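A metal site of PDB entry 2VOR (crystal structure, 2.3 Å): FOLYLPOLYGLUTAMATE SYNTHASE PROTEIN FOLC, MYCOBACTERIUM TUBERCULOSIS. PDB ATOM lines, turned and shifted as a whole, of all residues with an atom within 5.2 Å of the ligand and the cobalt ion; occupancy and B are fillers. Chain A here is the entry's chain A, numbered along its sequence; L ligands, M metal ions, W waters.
The backbone NH (N) of Thr 76 sits close to an oxygen (O5) of the ligand, 2.8 Å away. N of Ser 77 sits at hydrogen-bond distance from O7 of the ligand (3.3 Å). OG of Ser 77 is in hydrogen-bond range of O7 of the ligand, 2.6 Å away. NE of Arg 338 lies within salt-bridge range of O6 of the ligand (2.7 Å). An oxygen (O11) of the ligand lies within hydrogen-bond range of the side-chain carboxylate (OD1) of Asp 351 (2.8 Å). The backbone NH (N) of Lys 75 is in hydrogen-bond range of an oxygen (O4) of the ligand, 3.0 Å away. O4 of the ligand lies within salt-bridge range of NZ of Lys 75, 2.9 Å away. An oxygen (O8) of the ligand sits at hydrogen-bond distance from the backbone NH (N) of Gly 74, at 2.9 Å. A nitrogen (N2) of the ligand lies within hydrogen-bond range of the side-chain amide nitrogen (ND2) of Asn 301 (3.0 Å). An oxygen (O3) of the ligand is in hydrogen-bond range of a ring nitrogen (NE2) of His 354. An oxygen (O4) of the ligand sits close to the backbone carbonyl oxygen of Thr 72, at 3.0 Å. The backbone NH (N) of Ala 352 lies within hydrogen-bond range of an oxygen (O11) of the ligand, at 3.4 Å. ND2 of Asn 73 sits at hydrogen-bond distance from O10 of the ligand (3.4 Å).
OG of Ser 335 lies within hydrogen-bond range of OG of Ser 77. The backbone NH (N) of Ala 353 lies within hydrogen-bond range of the side-chain carboxylate (OD2) of Asp 351 (3.0 Å). OD1 of Asp 351 sits at hydrogen-bond distance from N of Leu 339 (2.8 Å). NZ of Lys 75 sits at hydrogen-bond distance from O of Gly 71, 3.2 Å away. The side-chain amide nitrogen (ND2) of Asn 301 is in hydrogen-bond range of the side-chain amide oxygen (OE1) of Gln 298, 3.0 Å away. The backbone NH of Thr 72 is in hydrogen-bond range of the backbone carbonyl oxygen of Pro 196, at 2.9 Å. N of Ala 352 sits at hydrogen-bond distance from O of Gly 337, 2.8 Å away. The backbone NH (N) of Asn 73 is in hydrogen-bond range of the backbone carbonyl oxygen (O) of Pro 196 (3.2 Å).
CD of Pro 99 touches O2 of the ligand, at 3.1 Å. His 297 touches the ligand. Ala 353 touches the ligand (N to O11, 3.7 Å). Gly 358 touches the ligand. Ala 361 touches the ligand. Val 472 touches the ligand. 19 residues have an atom within 4 Å of the ligand: Thr 72, Asn 73, Gly 74, Lys 75, Thr 76, Ser 77, Ser 98, Pro 99, Glu 174, His 297, Asn 301, Arg 338, Asp 351, Ala 352, Ala 353, His 354, Gly 358, Ala 361 and Val 472.
Residues that only touch the cobalt ion: Pro 99 (3.9 Å).
O1 of the ligand binds the cobalt ion, 2.0 Å away. O5 of the ligand binds the cobalt ion (2.1 Å). The cobalt ion is bound by the backbone carbonyl oxygen (O) of Ser 98 (2.2 Å). The cobalt ion is bound by the side-chain carboxylate (OE2) of Glu 174 (2.2 Å). OG1 of Thr 76 binds the cobalt ion.
Water W4 lies within hydrogen-bond range of NE2 of His 354 (3.0 Å), ND2 of Asn 73 (3.1 Å) and O of Thr 72 (3.1 Å). Water W2 lies within hydrogen-bond range of the backbone NH of His 354 (3.0 Å), the side-chain amide nitrogen of Asn 73 (3.1 Å) and an oxygen (O10) of the ligand (3.2 Å). Water W1 lies within hydrogen-bond range of a ring nitrogen (NE2) of His 297 (2.7 Å) and the side-chain amide nitrogen (NE2) of Gln 298 (3.3 Å).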
ATOM      1  N   GLY A  71      -6.801  24.263 -11.128  1.00  0.00           N
ATOM      2  CA  GLY A  71      -7.409  25.606 -11.299  1.00  0.00           C
ATOM      3  C   GLY A  71      -8.500  25.665 -10.276  1.00  0.00           C
ATOM      4  O   GLY A  71      -8.726  24.693  -9.545  1.00  0.00           O
ATOM      5  N   THR A  72      -9.200  26.787 -10.198  1.00  0.00           N
ATOM      6  CA  THR A  72     -10.250  26.906  -9.215  1.00  0.00           C
ATOM      7  C   THR A  72     -11.618  26.593  -9.825  1.00  0.00           C
ATOM      8  O   THR A  72     -12.464  25.905  -9.225  1.00  0.00           O
ATOM      9  CB  THR A  72     -10.314  28.364  -8.604  1.00  0.00           C
ATOM     10  OG1 THR A  72      -9.025  28.686  -8.018  1.00  0.00           O
ATOM     11  CG2 THR A  72     -11.389  28.481  -7.549  1.00  0.00           C
ATOM     12  N   ASN A  73     -11.866  27.136 -10.988  1.00  0.00           N
ATOM     13  CA  ASN A  73     -13.140  26.958 -11.636  1.00  0.00           C
ATOM     14  C   ASN A  73     -12.988  26.400 -13.056  1.00  0.00           C
ATOM     15  O   ASN A  73     -12.080  26.827 -13.821  1.00  0.00           O
ATOM     16  CB  ASN A  73     -13.811  28.270 -11.754  1.00  0.00           C
ATOM     17  CG  ASN A  73     -14.427  28.742 -10.420  1.00  0.00           C
ATOM     18  OD1 ASN A  73     -14.122  29.864  -9.979  1.00  0.00           O
ATOM     19  ND2 ASN A  73     -15.365  27.931  -9.823  1.00  0.00           N
ATOM     20  N   GLY A  74     -13.908  25.480 -13.430  1.00  0.00           N
ATOM     21  CA  GLY A  74     -14.014  25.044 -14.785  1.00  0.00           C
ATOM     22  C   GLY A  74     -13.204  23.825 -14.943  1.00  0.00           C
ATOM     23  O   GLY A  74     -13.126  23.336 -16.002  1.00  0.00           O
ATOM     24  N   LYS A  75     -12.624  23.267 -13.913  1.00  0.00           N
ATOM     25  CA  LYS A  75     -11.793  22.114 -14.206  1.00  0.00           C
ATOM     26  C   LYS A  75     -12.584  20.955 -14.779  1.00  0.00           C
ATOM     27  O   LYS A  75     -12.104  20.211 -15.674  1.00  0.00           O
ATOM     28  CB  LYS A  75     -10.983  21.581 -12.987  1.00  0.00           C
ATOM     29  CG  LYS A  75     -10.214  22.586 -12.135  1.00  0.00           C
ATOM     30  CD  LYS A  75      -9.368  21.781 -11.020  1.00  0.00           C
ATOM     31  CE  LYS A  75     -10.341  21.330  -9.883  1.00  0.00           C
ATOM     32  NZ  LYS A  75     -11.155  22.584  -9.444  1.00  0.00           N
ATOM     33  N   THR A  76     -13.739  20.697 -14.163  1.00  0.00           N
ATOM     34  CA  THR A  76     -14.617  19.576 -14.620  1.00  0.00           C
ATOM     35  C   THR A  76     -15.153  19.750 -16.020  1.00  0.00           C
ATOM     36  O   THR A  76     -15.042  18.882 -16.801  1.00  0.00           O
ATOM     37  CB  THR A  76     -15.793  19.253 -13.664  1.00  0.00           C
ATOM     38  OG1 THR A  76     -15.254  18.512 -12.593  1.00  0.00           O
ATOM     39  CG2 THR A  76     -16.849  18.322 -14.394  1.00  0.00           C
ATOM     40  N   SER A  77     -15.699  20.922 -16.295  1.00  0.00           N
ATOM     41  CA  SER A  77     -16.080  21.297 -17.593  1.00  0.00           C
ATOM     42  C   SER A  77     -15.019  21.135 -18.684  1.00  0.00           C
ATOM     43  O   SER A  77     -15.353  20.641 -19.752  1.00  0.00           O
ATOM     44  CB  SER A  77     -16.512  22.727 -17.584  1.00  0.00           C
ATOM     45  OG  SER A  77     -17.647  22.805 -16.793  1.00  0.00           O
ATOM     46  N   SER A  98     -13.745  15.183 -10.479  1.00  0.00           N
ATOM     47  CA  SER A  98     -14.241  15.274  -9.098  1.00  0.00           C
ATOM     48  C   SER A  98     -14.737  16.651  -8.836  1.00  0.00           C
ATOM     49  O   SER A  98     -14.467  17.579  -9.634  1.00  0.00           O
ATOM     50  CB  SER A  98     -13.200  14.877  -8.035  1.00  0.00           C
ATOM     51  OG  SER A  98     -12.050  15.677  -8.161  1.00  0.00           O
ATOM     52  N   PRO A  99     -15.579  16.782  -7.778  1.00  0.00           N
ATOM     53  CA  PRO A  99     -16.198  15.613  -7.110  1.00  0.00           C
ATOM     54  C   PRO A  99     -17.354  15.010  -7.944  1.00  0.00           C
ATOM     55  O   PRO A  99     -17.756  15.639  -8.915  1.00  0.00           O
ATOM     56  CB  PRO A  99     -16.845  16.228  -5.833  1.00  0.00           C
ATOM     57  CG  PRO A  99     -17.055  17.652  -6.107  1.00  0.00           C
ATOM     58  CD  PRO A  99     -16.186  18.072  -7.376  1.00  0.00           C
ATOM     59  N   GLU A 174      -8.380  15.394 -13.857  1.00  0.00           N
ATOM     60  CA  GLU A 174      -8.653  16.495 -12.976  1.00  0.00           C
ATOM     61  C   GLU A 174      -8.049  16.320 -11.551  1.00  0.00           C
ATOM     62  O   GLU A 174      -8.129  15.261 -10.903  1.00  0.00           O
ATOM     63  CB  GLU A 174     -10.181  16.683 -12.888  1.00  0.00           C
ATOM     64  CG  GLU A 174     -10.566  17.768 -11.995  1.00  0.00           C
ATOM     65  CD  GLU A 174     -12.068  17.924 -11.879  1.00  0.00           C
ATOM     66  OE1 GLU A 174     -12.889  17.231 -12.587  1.00  0.00           O
ATOM     67  OE2 GLU A 174     -12.426  18.776 -11.057  1.00  0.00           O
ATOM     68  N   PRO A 196      -9.072  29.210 -14.638  1.00  0.00           N
ATOM     69  CA  PRO A 196      -8.958  30.405 -13.783  1.00  0.00           C
ATOM     70  C   PRO A 196      -8.849  30.103 -12.273  1.00  0.00           C
ATOM     71  O   PRO A 196      -9.553  29.231 -11.739  1.00  0.00           O
ATOM     72  CB  PRO A 196     -10.193  31.192 -14.137  1.00  0.00           C
ATOM     73  CG  PRO A 196     -10.443  30.836 -15.640  1.00  0.00           C
ATOM     74  CD  PRO A 196     -10.089  29.365 -15.694  1.00  0.00           C
ATOM     75  N   HIS A 297     -18.449  32.131 -19.542  1.00  0.00           N
ATOM     76  CA  HIS A 297     -17.407  31.342 -18.957  1.00  0.00           C
ATOM     77  C   HIS A 297     -17.172  30.005 -19.686  1.00  0.00           C
ATOM     78  O   HIS A 297     -16.026  29.516 -19.753  1.00  0.00           O
ATOM     79  CB  HIS A 297     -17.645  31.121 -17.436  1.00  0.00           C
ATOM     80  CG  HIS A 297     -18.911  30.383 -17.108  1.00  0.00           C
ATOM     81  ND1 HIS A 297     -20.160  30.948 -17.245  1.00  0.00           N
ATOM     82  CD2 HIS A 297     -19.108  29.139 -16.628  1.00  0.00           C
ATOM     83  CE1 HIS A 297     -21.080  30.075 -16.885  1.00  0.00           C
ATOM     84  NE2 HIS A 297     -20.467  28.965 -16.516  1.00  0.00           N
ATOM     85  N   GLN A 298     -18.224  29.419 -20.267  1.00  0.00           N
ATOM     86  CA  GLN A 298     -18.061  28.141 -20.939  1.00  0.00           C
ATOM     87  C   GLN A 298     -17.376  28.357 -22.305  1.00  0.00           C
ATOM     88  O   GLN A 298     -16.783  27.447 -22.829  1.00  0.00           O
ATOM     89  CB  GLN A 298     -19.416  27.360 -21.077  1.00  0.00           C
ATOM     90  CG  GLN A 298     -20.018  26.896 -19.762  1.00  0.00           C
ATOM     91  CD  GLN A 298     -19.248  25.745 -19.145  1.00  0.00           C
ATOM     92  OE1 GLN A 298     -18.134  25.432 -19.540  1.00  0.00           O
ATOM     93  NE2 GLN A 298     -19.839  25.103 -18.151  1.00  0.00           N
ATOM     94  N   ASN A 301     -13.758  28.139 -21.118  1.00  0.00           N
ATOM     95  CA  ASN A 301     -13.470  26.710 -20.951  1.00  0.00           C
ATOM     96  C   ASN A 301     -13.296  26.031 -22.315  1.00  0.00           C
ATOM     97  O   ASN A 301     -12.342  25.295 -22.536  1.00  0.00           O
ATOM     98  CB  ASN A 301     -14.570  25.991 -20.080  1.00  0.00           C
ATOM     99  CG  ASN A 301     -14.616  26.513 -18.620  1.00  0.00           C
ATOM    100  OD1 ASN A 301     -13.603  27.027 -18.134  1.00  0.00           O
ATOM    101  ND2 ASN A 301     -15.763  26.361 -17.931  1.00  0.00           N
ATOM    102  N   SER A 335     -22.187  18.838 -19.583  1.00  0.00           N
ATOM    103  CA  SER A 335     -21.609  19.163 -18.277  1.00  0.00           C
ATOM    104  C   SER A 335     -22.737  19.183 -17.281  1.00  0.00           C
ATOM    105  O   SER A 335     -23.291  20.200 -16.982  1.00  0.00           O
ATOM    106  CB  SER A 335     -20.899  20.518 -18.293  1.00  0.00           C
ATOM    107  OG  SER A 335     -19.992  20.641 -17.165  1.00  0.00           O
ATOM    108  N   GLY A 337     -25.191  19.322 -14.191  1.00  0.00           N
ATOM    109  CA  GLY A 337     -25.192  20.190 -12.992  1.00  0.00           C
ATOM    110  C   GLY A 337     -24.415  21.485 -13.132  1.00  0.00           C
ATOM    111  O   GLY A 337     -24.182  22.179 -12.153  1.00  0.00           O
ATOM    112  N   ARG A 338     -23.962  21.810 -14.333  1.00  0.00           N
ATOM    113  CA  ARG A 338     -23.451  23.176 -14.643  1.00  0.00           C
ATOM    114  C   ARG A 338     -24.467  23.881 -15.582  1.00  0.00           C
ATOM    115  O   ARG A 338     -24.612  23.510 -16.782  1.00  0.00           O
ATOM    116  CB  ARG A 338     -22.046  23.125 -15.280  1.00  0.00           C
ATOM    117  CG  ARG A 338     -20.895  22.827 -14.271  1.00  0.00           C
ATOM    118  CD  ARG A 338     -21.101  21.407 -13.651  1.00  0.00           C
ATOM    119  NE  ARG A 338     -19.997  20.849 -12.850  1.00  0.00           N
ATOM    120  CZ  ARG A 338     -19.962  19.634 -12.284  1.00  0.00           C
ATOM    121  NH1 ARG A 338     -20.955  18.747 -12.439  1.00  0.00           N
ATOM    122  NH2 ARG A 338     -18.915  19.260 -11.560  1.00  0.00           N
ATOM    123  N   LEU A 339     -25.222  24.809 -15.017  1.00  0.00           N
ATOM    124  CA  LEU A 339     -26.354  25.475 -15.694  1.00  0.00           C
ATOM    125  C   LEU A 339     -27.120  24.489 -16.614  1.00  0.00           C
ATOM    126  O   LEU A 339     -27.241  24.681 -17.839  1.00  0.00           O
ATOM    127  CB  LEU A 339     -25.816  26.609 -16.502  1.00  0.00           C
ATOM    128  CG  LEU A 339     -26.339  28.042 -16.342  1.00  0.00           C
ATOM    129  CD1 LEU A 339     -27.517  28.117 -15.466  1.00  0.00           C
ATOM    130  CD2 LEU A 339     -25.173  28.936 -15.918  1.00  0.00           C
ATOM    131  N   ASP A 351     -27.212  24.385 -10.906  1.00  0.00           N
ATOM    132  CA  ASP A 351     -25.847  24.826 -11.179  1.00  0.00           C
ATOM    133  C   ASP A 351     -24.958  24.644  -9.991  1.00  0.00           C
ATOM    134  O   ASP A 351     -25.346  24.929  -8.903  1.00  0.00           O
ATOM    135  CB  ASP A 351     -25.777  26.249 -11.696  1.00  0.00           C
ATOM    136  CG  ASP A 351     -24.320  26.661 -12.046  1.00  0.00           C
ATOM    137  OD1 ASP A 351     -23.789  26.300 -13.118  1.00  0.00           O
ATOM    138  OD2 ASP A 351     -23.675  27.325 -11.200  1.00  0.00           O
ATOM    139  N   ALA A 352     -23.746  24.138 -10.184  1.00  0.00           N
ATOM    140  CA  ALA A 352     -22.913  23.700  -9.070  1.00  0.00           C
ATOM    141  C   ALA A 352     -22.111  24.847  -8.485  1.00  0.00           C
ATOM    142  O   ALA A 352     -21.110  24.587  -7.820  1.00  0.00           O
ATOM    143  CB  ALA A 352     -21.916  22.524  -9.566  1.00  0.00           C
ATOM    144  N   ALA A 353     -22.494  26.102  -8.743  1.00  0.00           N
ATOM    145  CA  ALA A 353     -21.725  27.302  -8.277  1.00  0.00           C
ATOM    146  C   ALA A 353     -21.507  27.303  -6.773  1.00  0.00           C
ATOM    147  O   ALA A 353     -22.445  27.302  -6.015  1.00  0.00           O
ATOM    148  CB  ALA A 353     -22.418  28.596  -8.703  1.00  0.00           C
ATOM    149  N   HIS A 354     -20.269  27.278  -6.330  1.00  0.00           N
ATOM    150  CA  HIS A 354     -19.993  27.187  -4.907  1.00  0.00           C
ATOM    151  C   HIS A 354     -18.881  28.131  -4.450  1.00  0.00           C
ATOM    152  O   HIS A 354     -18.274  27.931  -3.414  1.00  0.00           O
ATOM    153  CB  HIS A 354     -19.713  25.755  -4.462  1.00  0.00           C
ATOM    154  CG  HIS A 354     -18.613  25.062  -5.206  1.00  0.00           C
ATOM    155  ND1 HIS A 354     -17.268  25.271  -4.928  1.00  0.00           N
ATOM    156  CD2 HIS A 354     -18.651  24.092  -6.156  1.00  0.00           C
ATOM    157  CE1 HIS A 354     -16.535  24.483  -5.697  1.00  0.00           C
ATOM    158  NE2 HIS A 354     -17.359  23.789  -6.472  1.00  0.00           N
ATOM    159  N   ALA A 357     -16.641  33.663  -7.685  1.00  0.00           N
ATOM    160  CA  ALA A 357     -16.401  33.754  -9.109  1.00  0.00           C
ATOM    161  C   ALA A 357     -17.422  32.881  -9.858  1.00  0.00           C
ATOM    162  O   ALA A 357     -17.981  33.314 -10.855  1.00  0.00           O
ATOM    163  CB  ALA A 357     -14.966  33.308  -9.414  1.00  0.00           C
ATOM    164  N   GLY A 358     -17.702  31.682  -9.377  1.00  0.00           N
ATOM    165  CA  GLY A 358     -18.720  30.762  -9.992  1.00  0.00           C
ATOM    166  C   GLY A 358     -20.138  31.340  -9.885  1.00  0.00           C
ATOM    167  O   GLY A 358     -20.901  31.320 -10.836  1.00  0.00           O
ATOM    168  N   ALA A 359     -20.473  31.843  -8.725  1.00  0.00           N
ATOM    169  CA  ALA A 359     -21.761  32.508  -8.396  1.00  0.00           C
ATOM    170  C   ALA A 359     -22.004  33.755  -9.295  1.00  0.00           C
ATOM    171  O   ALA A 359     -23.127  34.074  -9.774  1.00  0.00           O
ATOM    172  CB  ALA A 359     -21.728  32.902  -6.887  1.00  0.00           C
ATOM    173  N   ALA A 361     -20.505  34.200 -12.244  1.00  0.00           N
ATOM    174  CA  ALA A 361     -20.621  33.700 -13.625  1.00  0.00           C
ATOM    175  C   ALA A 361     -22.033  33.157 -13.832  1.00  0.00           C
ATOM    176  O   ALA A 361     -22.664  33.424 -14.843  1.00  0.00           O
ATOM    177  CB  ALA A 361     -19.527  32.625 -13.940  1.00  0.00           C
ATOM    178  N   LEU A 362     -22.567  32.460 -12.828  1.00  0.00           N
ATOM    179  CA  LEU A 362     -23.951  32.086 -12.875  1.00  0.00           C
ATOM    180  C   LEU A 362     -24.932  33.296 -13.023  1.00  0.00           C
ATOM    181  O   LEU A 362     -25.800  33.249 -13.863  1.00  0.00           O
ATOM    182  CB  LEU A 362     -24.291  31.219 -11.658  1.00  0.00           C
ATOM    183  CG  LEU A 362     -25.800  30.951 -11.484  1.00  0.00           C
ATOM    184  CD1 LEU A 362     -26.193  30.079 -12.706  1.00  0.00           C
ATOM    185  CD2 LEU A 362     -26.197  30.275 -10.114  1.00  0.00           C
ATOM    186  N   VAL A 472     -21.955  21.444  -5.371  1.00  0.00           N
ATOM    187  CA  VAL A 472     -21.963  20.273  -6.206  1.00  0.00           C
ATOM    188  C   VAL A 472     -22.934  19.272  -5.649  1.00  0.00           C
ATOM    189  O   VAL A 472     -23.644  18.569  -6.414  1.00  0.00           O
ATOM    190  CB  VAL A 472     -20.612  19.581  -6.158  1.00  0.00           C
ATOM    191  CG1 VAL A 472     -20.680  18.197  -6.813  1.00  0.00           C
ATOM    192  CG2 VAL A 472     -19.610  20.441  -6.826  1.00  0.00           C
HETATM  193  P1  LIG L   1     -16.295  21.533  -8.914  1.00  0.00           P
HETATM  194  O1  LIG L   1     -16.235  20.316 -10.251  1.00  0.00           O
HETATM  195  O2  LIG L   1     -15.767  21.147  -7.515  1.00  0.00           O
HETATM  196  O3  LIG L   1     -17.711  22.023  -8.919  1.00  0.00           O
HETATM  197  P2  LIG L   1     -14.595  22.829 -11.062  1.00  0.00           P
HETATM  198  O4  LIG L   1     -13.337  23.602 -11.020  1.00  0.00           O
HETATM  199  O5  LIG L   1     -14.304  21.439 -11.486  1.00  0.00           O
HETATM  200  C1  LIG L   1     -14.927  22.690  -9.251  1.00  0.00           C
HETATM  201  P3  LIG L   1     -16.643  22.948 -12.889  1.00  0.00           P
HETATM  202  O6  LIG L   1     -17.676  22.048 -12.102  1.00  0.00           O
HETATM  203  O7  LIG L   1     -16.896  23.288 -14.337  1.00  0.00           O
HETATM  204  O8  LIG L   1     -15.617  23.720 -11.846  1.00  0.00           O
HETATM  205  O9  LIG L   1     -17.697  24.271 -12.562  1.00  0.00           O
HETATM  206  C2  LIG L   1     -18.259  24.639 -11.217  1.00  0.00           C
HETATM  207  C3  LIG L   1     -19.106  25.890 -11.266  1.00  0.00           C
HETATM  208  O10 LIG L   1     -18.144  26.921 -11.594  1.00  0.00           O
HETATM  209  C4  LIG L   1     -20.007  25.864 -12.498  1.00  0.00           C
HETATM  210  O11 LIG L   1     -21.311  25.392 -12.209  1.00  0.00           O
HETATM  211  C5  LIG L   1     -20.093  27.319 -12.949  1.00  0.00           C
HETATM  212  O12 LIG L   1     -21.022  28.066 -12.158  1.00  0.00           O
HETATM  213  C6  LIG L   1     -18.738  27.855 -12.564  1.00  0.00           C
HETATM  214  N1  LIG L   1     -17.665  27.911 -13.600  1.00  0.00           N
HETATM  215  C7  LIG L   1     -17.221  26.921 -14.441  1.00  0.00           C
HETATM  216  N2  LIG L   1     -16.190  27.370 -15.186  1.00  0.00           N
HETATM  217  C8  LIG L   1     -16.013  28.660 -14.830  1.00  0.00           C
HETATM  218  C9  LIG L   1     -15.113  29.629 -15.223  1.00  0.00           C
HETATM  219  N3  LIG L   1     -14.204  29.374 -16.165  1.00  0.00           N
HETATM  220  N4  LIG L   1     -15.178  30.815 -14.615  1.00  0.00           N
HETATM  221  C10 LIG L   1     -16.093  31.114 -13.706  1.00  0.00           C
HETATM  222  N5  LIG L   1     -16.971  30.214 -13.293  1.00  0.00           N
HETATM  223  C11 LIG L   1     -16.922  28.990 -13.824  1.00  0.00           C
HETATM  224 CO    CO M   1     -14.471  19.513 -10.594  1.00  0.00          CO
HETATM  225  O   HOH W   1     -21.726  26.600 -15.959  1.00  0.00           O
HETATM  226  O   HOH W   2     -18.093  27.394  -8.408  1.00  0.00           O
HETATM  227  O   HOH W   3     -13.742  32.395 -17.595  1.00  0.00           O
HETATM  228  O   HOH W   4     -15.368  25.215  -8.252  1.00  0.00           O
HETATM  229  O   HOH W   5     -13.421  33.122 -14.316  1.00  0.00           O
